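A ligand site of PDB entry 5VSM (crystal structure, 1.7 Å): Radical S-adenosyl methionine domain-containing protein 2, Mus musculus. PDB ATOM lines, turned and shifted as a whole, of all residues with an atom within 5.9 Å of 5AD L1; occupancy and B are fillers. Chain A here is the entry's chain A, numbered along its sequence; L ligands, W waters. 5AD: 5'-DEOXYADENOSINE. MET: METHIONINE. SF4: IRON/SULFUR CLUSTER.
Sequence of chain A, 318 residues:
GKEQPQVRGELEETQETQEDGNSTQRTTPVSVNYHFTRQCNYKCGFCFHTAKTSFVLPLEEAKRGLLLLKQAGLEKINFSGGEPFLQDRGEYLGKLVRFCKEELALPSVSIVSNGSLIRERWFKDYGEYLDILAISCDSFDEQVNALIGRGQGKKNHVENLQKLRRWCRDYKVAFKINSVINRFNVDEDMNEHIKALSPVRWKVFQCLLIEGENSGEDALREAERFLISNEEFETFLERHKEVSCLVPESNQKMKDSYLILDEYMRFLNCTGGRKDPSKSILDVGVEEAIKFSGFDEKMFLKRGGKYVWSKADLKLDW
An oxygen (O3') of 5AD L1 lies within hydrogen-bond range of the side-chain hydroxyl (OG) of Ser 136 (2.7 Å).
The guanidinium group of Arg 150 is in hydrogen-bond range of an oxygen (O2') of 5AD L1, 2.8 Å away.
The backbone carbonyl oxygen (O) of Phe 46 sits at hydrogen-bond distance from a nitrogen (N6) of 5AD L1.
The backbone NH of Leu 208 sits at hydrogen-bond distance from a nitrogen (N1) of 5AD L1, 2.8 Å away.
The backbone carbonyl oxygen (O) of Leu 208 is in hydrogen-bond range of a nitrogen (N6) of 5AD L1 (3.1 Å).
The side-chain amide nitrogen (ND2) of Asn 178 sits at hydrogen-bond distance from an oxygen (O3') of 5AD L1, at 3.1 Å.
A nitrogen (N7) of 5AD L1 lies close to the backbone NH (N) of Phe 48, 3.4 Å away.
The side-chain amide nitrogen (ND2) of Asn 214 sits close to a nitrogen (N6) of 5AD L1 (3.4 Å).
The side-chain hydroxyl (OG) of Ser 136 sits at hydrogen-bond distance from an oxygen (OXT) of MET L2 (2.4 Å).
The guanidinium group of Arg 150 sits close to an oxygen (O) of MET L2, 2.9 Å away.
The guanidinium group (NH1) of Arg 150 lies close to a sulfur (S3) of SF4 L3.
An iron atom (FE3) of SF4 L3 is bound by the side-chain sulfur of Cys 47.
An iron atom (FE4) of SF4 L3 is bound by an oxygen (O) of MET L2 (2.3 Å).
The side-chain carboxylate of Asp 138 is in salt-bridge range of the guanidinium group of Arg 150 (2.8 Å).
ND2 of Asn 214 lies within hydrogen-bond range of O of Phe 46 (2.8 Å).
The backbone carbonyl oxygen of Leu 208 sits at hydrogen-bond distance from the side-chain amide nitrogen of Asn 214 (2.9 Å).
OD1 of Asp 138 is in hydrogen-bond range of N of Val 180 (2.8 Å).
N of Ala 223 sits at hydrogen-bond distance from O of Asn 214 (2.8 Å).
O of Ser 179 sits at hydrogen-bond distance from N of Phe 205 (2.8 Å).
The backbone carbonyl oxygen (O) of His 49 sits close to the side-chain sulfur (SG) of Cys 47 (3.4 Å).
Cys 47 touches 5AD L1 (CA to N7, 3.8 Å).
Ser 80 touches 5AD L1.
Val 112 touches 5AD L1.
CG2 of Val 180 touches C4 of 5AD L1, at 3.3 Å.
Phe 205 touches 5AD L1 (CB to N3, 3.8 Å).
O of Gln 206 touches C2 of 5AD L1 (3.5 Å).
Cys 207 touches 5AD L1 (CA to N1, 3.6 Å).
Hydrophobic or aromatic side chains within 4 Å of 5AD L1: Phe 46, Phe 48, Val 112, Val 180, Phe 205 and Leu 208.
14 residues have an atom within 4 Å of 5AD L1: Phe 46, Cys 47, Phe 48, Ser 80, Val 112, Ser 136, Arg 150, Asn 178, Val 180, Phe 205, Gln 206, Cys 207, Leu 208 and Asn 214.
Water W1 lies within hydrogen-bond range of O2' of 5AD L1 (2.7 Å), OD1 of Asp 138 (2.8 Å), O of Asn 178 (3.0 Å), NH2 of Arg 150 (3.0 Å) and N of Val 180 (3.4 Å).
Water W2 lies within hydrogen-bond range of OH of Tyr 258 and OG of Ser 80.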
ATOM      1  N   HIS A  35      28.771  15.212  -0.371  1.00  0.00           N
ATOM      2  CA  HIS A  35      27.705  15.433  -1.360  1.00  0.00           C
ATOM      3  C   HIS A  35      27.997  14.536  -2.553  1.00  0.00           C
ATOM      4  O   HIS A  35      28.540  14.954  -3.583  1.00  0.00           O
ATOM      5  CB  HIS A  35      27.626  16.910  -1.741  1.00  0.00           C
ATOM      6  CG  HIS A  35      27.241  17.806  -0.601  1.00  0.00           C
ATOM      7  ND1 HIS A  35      26.037  18.475  -0.551  1.00  0.00           N
ATOM      8  CD2 HIS A  35      27.890  18.123   0.543  1.00  0.00           C
ATOM      9  CE1 HIS A  35      25.958  19.167   0.573  1.00  0.00           C
ATOM     10  NE2 HIS A  35      27.077  18.974   1.248  1.00  0.00           N
ATOM     11  N   PHE A  46      15.995  27.973  -3.709  1.00  0.00           N
ATOM     12  CA  PHE A  46      17.236  28.465  -3.113  1.00  0.00           C
ATOM     13  C   PHE A  46      18.371  27.443  -3.133  1.00  0.00           C
ATOM     14  O   PHE A  46      19.455  27.761  -2.656  1.00  0.00           O
ATOM     15  CB  PHE A  46      16.993  28.888  -1.667  1.00  0.00           C
ATOM     16  CG  PHE A  46      16.255  27.868  -0.849  1.00  0.00           C
ATOM     17  CD1 PHE A  46      16.874  26.660  -0.487  1.00  0.00           C
ATOM     18  CD2 PHE A  46      14.967  28.117  -0.418  1.00  0.00           C
ATOM     19  CE1 PHE A  46      16.195  25.703   0.262  1.00  0.00           C
ATOM     20  CE2 PHE A  46      14.279  27.170   0.339  1.00  0.00           C
ATOM     21  CZ  PHE A  46      14.903  25.963   0.677  1.00  0.00           C
ATOM     22  N   CYS A  47      18.151  26.255  -3.676  1.00  0.00           N
ATOM     23  CA  CYS A  47      19.089  25.137  -3.550  1.00  0.00           C
ATOM     24  C   CYS A  47      20.535  25.566  -3.811  1.00  0.00           C
ATOM     25  O   CYS A  47      20.840  26.110  -4.872  1.00  0.00           O
ATOM     26  CB  CYS A  47      18.703  24.021  -4.524  1.00  0.00           C
ATOM     27  SG  CYS A  47      19.892  22.648  -4.470  1.00  0.00           S
ATOM     28  N   PHE A  48      21.441  25.337  -2.843  1.00  0.00           N
ATOM     29  CA  PHE A  48      22.811  25.784  -3.032  1.00  0.00           C
ATOM     30  C   PHE A  48      23.780  24.664  -3.408  1.00  0.00           C
ATOM     31  O   PHE A  48      24.994  24.909  -3.437  1.00  0.00           O
ATOM     32  CB  PHE A  48      23.322  26.566  -1.809  1.00  0.00           C
ATOM     33  CG  PHE A  48      23.487  25.775  -0.529  1.00  0.00           C
ATOM     34  CD1 PHE A  48      24.010  26.406   0.589  1.00  0.00           C
ATOM     35  CD2 PHE A  48      23.130  24.442  -0.422  1.00  0.00           C
ATOM     36  CE1 PHE A  48      24.182  25.726   1.792  1.00  0.00           C
ATOM     37  CE2 PHE A  48      23.288  23.751   0.764  1.00  0.00           C
ATOM     38  CZ  PHE A  48      23.821  24.395   1.877  1.00  0.00           C
ATOM     39  N   HIS A  49      23.287  23.480  -3.752  1.00  0.00           N
ATOM     40  CA  HIS A  49      24.134  22.401  -4.268  1.00  0.00           C
ATOM     41  C   HIS A  49      23.343  21.722  -5.385  1.00  0.00           C
ATOM     42  O   HIS A  49      22.648  20.736  -5.157  1.00  0.00           O
ATOM     43  CB  HIS A  49      24.543  21.416  -3.189  1.00  0.00           C
ATOM     44  CG  HIS A  49      25.804  20.674  -3.518  1.00  0.00           C
ATOM     45  ND1 HIS A  49      27.048  21.248  -3.381  1.00  0.00           N
ATOM     46  CD2 HIS A  49      26.012  19.439  -4.021  1.00  0.00           C
ATOM     47  CE1 HIS A  49      27.971  20.393  -3.780  1.00  0.00           C
ATOM     48  NE2 HIS A  49      27.369  19.283  -4.164  1.00  0.00           N
ATOM     49  N   SER A  80      25.081  13.599   1.882  1.00  0.00           N
ATOM     50  CA  SER A  80      24.269  14.715   1.410  1.00  0.00           C
ATOM     51  C   SER A  80      24.252  14.709  -0.124  1.00  0.00           C
ATOM     52  O   SER A  80      24.685  13.749  -0.770  1.00  0.00           O
ATOM     53  CB  SER A  80      24.803  16.035   1.956  1.00  0.00           C
ATOM     54  OG  SER A  80      23.823  17.049   1.800  1.00  0.00           O
ATOM     55  N   VAL A 112      21.407  13.532   5.441  1.00  0.00           N
ATOM     56  CA  VAL A 112      20.449  14.624   5.326  1.00  0.00           C
ATOM     57  C   VAL A 112      19.668  14.424   4.031  1.00  0.00           C
ATOM     58  O   VAL A 112      20.252  14.241   2.966  1.00  0.00           O
ATOM     59  CB  VAL A 112      21.130  16.012   5.375  1.00  0.00           C
ATOM     60  CG1 VAL A 112      22.258  16.108   4.354  1.00  0.00           C
ATOM     61  CG2 VAL A 112      20.108  17.117   5.151  1.00  0.00           C
ATOM     62  N   SER A 136      14.952  17.597   5.816  1.00  0.00           N
ATOM     63  CA  SER A 136      14.838  19.023   5.517  1.00  0.00           C
ATOM     64  C   SER A 136      13.373  19.406   5.367  1.00  0.00           C
ATOM     65  O   SER A 136      12.667  18.857   4.511  1.00  0.00           O
ATOM     66  CB  SER A 136      15.613  19.347   4.255  1.00  0.00           C
ATOM     67  OG  SER A 136      17.013  19.209   4.480  1.00  0.00           O
ATOM     68  N   ASP A 138      11.200  23.166   5.583  1.00  0.00           N
ATOM     69  CA  ASP A 138      11.362  24.588   5.828  1.00  0.00           C
ATOM     70  C   ASP A 138      10.108  25.259   6.385  1.00  0.00           C
ATOM     71  O   ASP A 138      10.193  26.389   6.885  1.00  0.00           O
ATOM     72  CB  ASP A 138      11.774  25.283   4.529  1.00  0.00           C
ATOM     73  CG  ASP A 138      12.931  24.568   3.871  1.00  0.00           C
ATOM     74  OD1 ASP A 138      13.968  24.353   4.549  1.00  0.00           O
ATOM     75  OD2 ASP A 138      12.786  24.182   2.702  1.00  0.00           O
ATOM     76  N   ARG A 150       9.998  22.817  -2.431  1.00  0.00           N
ATOM     77  CA  ARG A 150      10.308  21.699  -1.541  1.00  0.00           C
ATOM     78  C   ARG A 150       9.168  20.685  -1.689  1.00  0.00           C
ATOM     79  O   ARG A 150       8.310  20.503  -0.821  1.00  0.00           O
ATOM     80  CB  ARG A 150      10.476  22.201  -0.108  1.00  0.00           C
ATOM     81  CG  ARG A 150      10.852  21.130   0.927  1.00  0.00           C
ATOM     82  CD  ARG A 150      12.320  20.748   0.865  1.00  0.00           C
ATOM     83  NE  ARG A 150      13.185  21.743   1.481  1.00  0.00           N
ATOM     84  CZ  ARG A 150      14.507  21.615   1.587  1.00  0.00           C
ATOM     85  NH1 ARG A 150      15.104  20.539   1.099  1.00  0.00           N
ATOM     86  NH2 ARG A 150      15.230  22.555   2.176  1.00  0.00           N
ATOM     87  N   ASN A 178      16.109  19.872   9.600  1.00  0.00           N
ATOM     88  CA  ASN A 178      16.845  21.019   9.071  1.00  0.00           C
ATOM     89  C   ASN A 178      15.827  21.946   8.399  1.00  0.00           C
ATOM     90  O   ASN A 178      14.966  21.483   7.660  1.00  0.00           O
ATOM     91  CB  ASN A 178      17.873  20.634   8.009  1.00  0.00           C
ATOM     92  CG  ASN A 178      19.063  19.839   8.560  1.00  0.00           C
ATOM     93  OD1 ASN A 178      19.134  19.506   9.753  1.00  0.00           O
ATOM     94  ND2 ASN A 178      20.016  19.554   7.691  1.00  0.00           N
ATOM     95  N   SER A 179      15.956  23.240   8.656  1.00  0.00           N
ATOM     96  CA  SER A 179      15.101  24.229   8.012  1.00  0.00           C
ATOM     97  C   SER A 179      15.980  25.331   7.438  1.00  0.00           C
ATOM     98  O   SER A 179      16.918  25.785   8.109  1.00  0.00           O
ATOM     99  CB  SER A 179      14.096  24.823   9.004  1.00  0.00           C
ATOM    100  OG  SER A 179      13.275  23.812   9.584  1.00  0.00           O
ATOM    101  N   VAL A 180      15.688  25.758   6.204  1.00  0.00           N
ATOM    102  CA  VAL A 180      16.355  26.905   5.594  1.00  0.00           C
ATOM    103  C   VAL A 180      15.468  28.118   5.820  1.00  0.00           C
ATOM    104  O   VAL A 180      14.322  28.143   5.370  1.00  0.00           O
ATOM    105  CB  VAL A 180      16.611  26.691   4.081  1.00  0.00           C
ATOM    106  CG1 VAL A 180      17.246  27.960   3.491  1.00  0.00           C
ATOM    107  CG2 VAL A 180      17.499  25.473   3.864  1.00  0.00           C
ATOM    108  N   PHE A 205      19.246  26.967   9.178  1.00  0.00           N
ATOM    109  CA  PHE A 205      20.217  27.575   8.281  1.00  0.00           C
ATOM    110  C   PHE A 205      19.669  28.896   7.760  1.00  0.00           C
ATOM    111  O   PHE A 205      18.551  28.950   7.250  1.00  0.00           O
ATOM    112  CB  PHE A 205      20.505  26.689   7.071  1.00  0.00           C
ATOM    113  CG  PHE A 205      21.071  25.341   7.408  1.00  0.00           C
ATOM    114  CD1 PHE A 205      22.435  25.104   7.263  1.00  0.00           C
ATOM    115  CD2 PHE A 205      20.260  24.298   7.814  1.00  0.00           C
ATOM    116  CE1 PHE A 205      22.975  23.867   7.554  1.00  0.00           C
ATOM    117  CE2 PHE A 205      20.810  23.047   8.106  1.00  0.00           C
ATOM    118  CZ  PHE A 205      22.165  22.833   7.964  1.00  0.00           C
ATOM    119  N   GLN A 206      20.472  29.957   7.861  1.00  0.00           N
ATOM    120  CA  GLN A 206      20.172  31.166   7.094  1.00  0.00           C
ATOM    121  C   GLN A 206      20.381  30.886   5.610  1.00  0.00           C
ATOM    122  O   GLN A 206      21.388  30.290   5.219  1.00  0.00           O
ATOM    123  CB  GLN A 206      21.070  32.297   7.560  1.00  0.00           C
ATOM    124  CG  GLN A 206      20.843  33.631   6.817  1.00  0.00           C
ATOM    125  CD  GLN A 206      21.748  34.728   7.320  1.00  0.00           C
ATOM    126  OE1 GLN A 206      22.686  34.478   8.069  1.00  0.00           O
ATOM    127  NE2 GLN A 206      21.479  35.961   6.915  1.00  0.00           N
ATOM    128  N   CYS A 207      19.438  31.308   4.764  1.00  0.00           N
ATOM    129  CA  CYS A 207      19.567  31.060   3.328  1.00  0.00           C
ATOM    130  C   CYS A 207      20.900  31.597   2.824  1.00  0.00           C
ATOM    131  O   CYS A 207      21.264  32.747   3.102  1.00  0.00           O
ATOM    132  CB  CYS A 207      18.409  31.716   2.582  1.00  0.00           C
ATOM    133  SG  CYS A 207      18.322  31.183   0.831  1.00  0.00           S
ATOM    134  N   LEU A 208      21.664  30.762   2.126  1.00  0.00           N
ATOM    135  CA  LEU A 208      23.027  31.098   1.744  1.00  0.00           C
ATOM    136  C   LEU A 208      23.162  31.182   0.232  1.00  0.00           C
ATOM    137  O   LEU A 208      22.737  30.283  -0.499  1.00  0.00           O
ATOM    138  CB  LEU A 208      24.026  30.075   2.304  1.00  0.00           C
ATOM    139  CG  LEU A 208      25.499  30.309   1.969  1.00  0.00           C
ATOM    140  CD1 LEU A 208      26.002  31.575   2.619  1.00  0.00           C
ATOM    141  CD2 LEU A 208      26.346  29.124   2.428  1.00  0.00           C
ATOM    142  N   LEU A 209      23.776  32.270  -0.238  1.00  0.00           N
ATOM    143  CA  LEU A 209      24.081  32.442  -1.649  1.00  0.00           C
ATOM    144  C   LEU A 209      25.485  31.928  -1.930  1.00  0.00           C
ATOM    145  O   LEU A 209      26.438  32.276  -1.220  1.00  0.00           O
ATOM    146  CB  LEU A 209      23.969  33.918  -2.037  1.00  0.00           C
ATOM    147  CG  LEU A 209      23.636  34.264  -3.487  1.00  0.00           C
ATOM    148  CD1 LEU A 209      22.247  33.755  -3.781  1.00  0.00           C
ATOM    149  CD2 LEU A 209      23.713  35.773  -3.681  1.00  0.00           C
ATOM    150  N   ASN A 214      23.633  28.882  -6.800  1.00  0.00           N
ATOM    151  CA  ASN A 214      22.314  29.520  -6.804  1.00  0.00           C
ATOM    152  C   ASN A 214      22.428  31.021  -7.057  1.00  0.00           C
ATOM    153  O   ASN A 214      21.559  31.796  -6.634  1.00  0.00           O
ATOM    154  CB  ASN A 214      21.556  29.225  -5.516  1.00  0.00           C
ATOM    155  CG  ASN A 214      22.294  29.694  -4.277  1.00  0.00           C
ATOM    156  OD1 ASN A 214      23.335  30.349  -4.369  1.00  0.00           O
ATOM    157  ND2 ASN A 214      21.756  29.380  -3.104  1.00  0.00           N
ATOM    158  N   ALA A 223      18.834  32.398  -6.222  1.00  0.00           N
ATOM    159  CA  ALA A 223      18.277  32.430  -4.875  1.00  0.00           C
ATOM    160  C   ALA A 223      18.176  33.835  -4.293  1.00  0.00           C
ATOM    161  O   ALA A 223      17.719  33.967  -3.154  1.00  0.00           O
ATOM    162  CB  ALA A 223      19.115  31.535  -3.959  1.00  0.00           C
ATOM    163  N   MET A 254      28.381  28.982   8.260  1.00  0.00           N
ATOM    164  CA  MET A 254      28.504  28.045   7.147  1.00  0.00           C
ATOM    165  C   MET A 254      29.786  28.290   6.373  1.00  0.00           C
ATOM    166  O   MET A 254      30.505  27.338   6.041  1.00  0.00           O
ATOM    167  CB  MET A 254      27.277  28.171   6.230  1.00  0.00           C
ATOM    168  CG  MET A 254      26.074  27.579   6.960  1.00  0.00           C
ATOM    169  SD  MET A 254      26.102  25.756   6.899  1.00  0.00           S
ATOM    170  CE  MET A 254      25.785  25.427   5.139  1.00  0.00           C
ATOM    171  N   TYR A 258      31.598  24.796   7.238  1.00  0.00           N
ATOM    172  CA  TYR A 258      30.929  23.761   6.452  1.00  0.00           C
ATOM    173  C   TYR A 258      31.842  23.341   5.298  1.00  0.00           C
ATOM    174  O   TYR A 258      32.036  24.100   4.340  1.00  0.00           O
ATOM    175  CB  TYR A 258      29.573  24.257   5.946  1.00  0.00           C
ATOM    176  CG  TYR A 258      28.721  23.148   5.365  1.00  0.00           C
ATOM    177  CD1 TYR A 258      27.829  22.451   6.170  1.00  0.00           C
ATOM    178  CD2 TYR A 258      28.828  22.788   4.032  1.00  0.00           C
ATOM    179  CE1 TYR A 258      27.048  21.442   5.657  1.00  0.00           C
ATOM    180  CE2 TYR A 258      28.056  21.771   3.513  1.00  0.00           C
ATOM    181  CZ  TYR A 258      27.166  21.091   4.327  1.00  0.00           C
ATOM    182  OH  TYR A 258      26.392  20.078   3.800  1.00  0.00           O
HETATM  183  N1  5AD L   1      21.082  27.998   2.208  1.00  0.00           N
HETATM  184  C2  5AD L   1      21.174  27.309   3.327  1.00  0.00           C
HETATM  185  N3  5AD L   1      20.862  26.026   3.395  1.00  0.00           N
HETATM  186  C4  5AD L   1      20.459  25.378   2.313  1.00  0.00           C
HETATM  187  N9  5AD L   1      20.070  24.101   2.082  1.00  0.00           N
HETATM  188  C8  5AD L   1      19.746  23.983   0.755  1.00  0.00           C
HETATM  189  N7  5AD L   1      19.893  25.151   0.156  1.00  0.00           N
HETATM  190  C5  5AD L   1      20.334  26.060   1.091  1.00  0.00           C
HETATM  191  C6  5AD L   1      20.680  27.416   1.070  1.00  0.00           C
HETATM  192  N6  5AD L   1      20.564  28.137  -0.119  1.00  0.00           N
HETATM  193  C1' 5AD L   1      20.073  23.080   3.139  1.00  0.00           C
HETATM  194  C2' 5AD L   1      19.219  21.837   2.798  1.00  0.00           C
HETATM  195  C3' 5AD L   1      19.828  20.784   3.773  1.00  0.00           C
HETATM  196  C4' 5AD L   1      21.257  21.317   4.014  1.00  0.00           C
HETATM  197  C5' 5AD L   1      22.299  20.319   3.482  1.00  0.00           C
HETATM  198  O4' 5AD L   1      21.390  22.511   3.208  1.00  0.00           O
HETATM  199  O2' 5AD L   1      17.840  22.110   3.049  1.00  0.00           O
HETATM  200  O3' 5AD L   1      19.112  20.777   5.011  1.00  0.00           O
HETATM  201  N   MET L   2      18.572  17.100  -0.710  1.00  0.00           N
HETATM  202  CA  MET L   2      18.891  16.997   0.723  1.00  0.00           C
HETATM  203  C   MET L   2      18.013  17.965   1.486  1.00  0.00           C
HETATM  204  O   MET L   2      17.522  18.967   1.000  1.00  0.00           O
HETATM  205  CB  MET L   2      20.369  17.267   1.045  1.00  0.00           C
HETATM  206  CG  MET L   2      21.102  18.205   0.085  1.00  0.00           C
HETATM  207  SD  MET L   2      20.410  19.879   0.132  1.00  0.00           S
HETATM  208  CE  MET L   2      21.457  20.722  -1.101  1.00  0.00           C
HETATM  209  OXT MET L   2      17.766  17.712   2.755  1.00  0.00           O
HETATM  210 FE1  SF4 L   3      17.033  18.911  -3.715  1.00  0.00          FE
HETATM  211 FE2  SF4 L   3      15.959  20.929  -2.371  1.00  0.00          FE
HETATM  212 FE3  SF4 L   3      18.433  21.115  -3.350  1.00  0.00          FE
HETATM  213 FE4  SF4 L   3      18.063  19.358  -1.179  1.00  0.00          FE
HETATM  214  S1  SF4 L   3      17.748  21.740  -1.307  1.00  0.00           S
HETATM  215  S2  SF4 L   3      19.183  19.013  -3.251  1.00  0.00           S
HETATM  216  S3  SF4 L   3      15.792  18.782  -1.735  1.00  0.00           S
HETATM  217  S4  SF4 L   3      16.506  20.908  -4.583  1.00  0.00           S
HETATM  218  O   HOH W   1      16.081  22.529   5.093  1.00  0.00           O
HETATM  219  O   HOH W   2      24.696  18.342   4.587  1.00  0.00           O
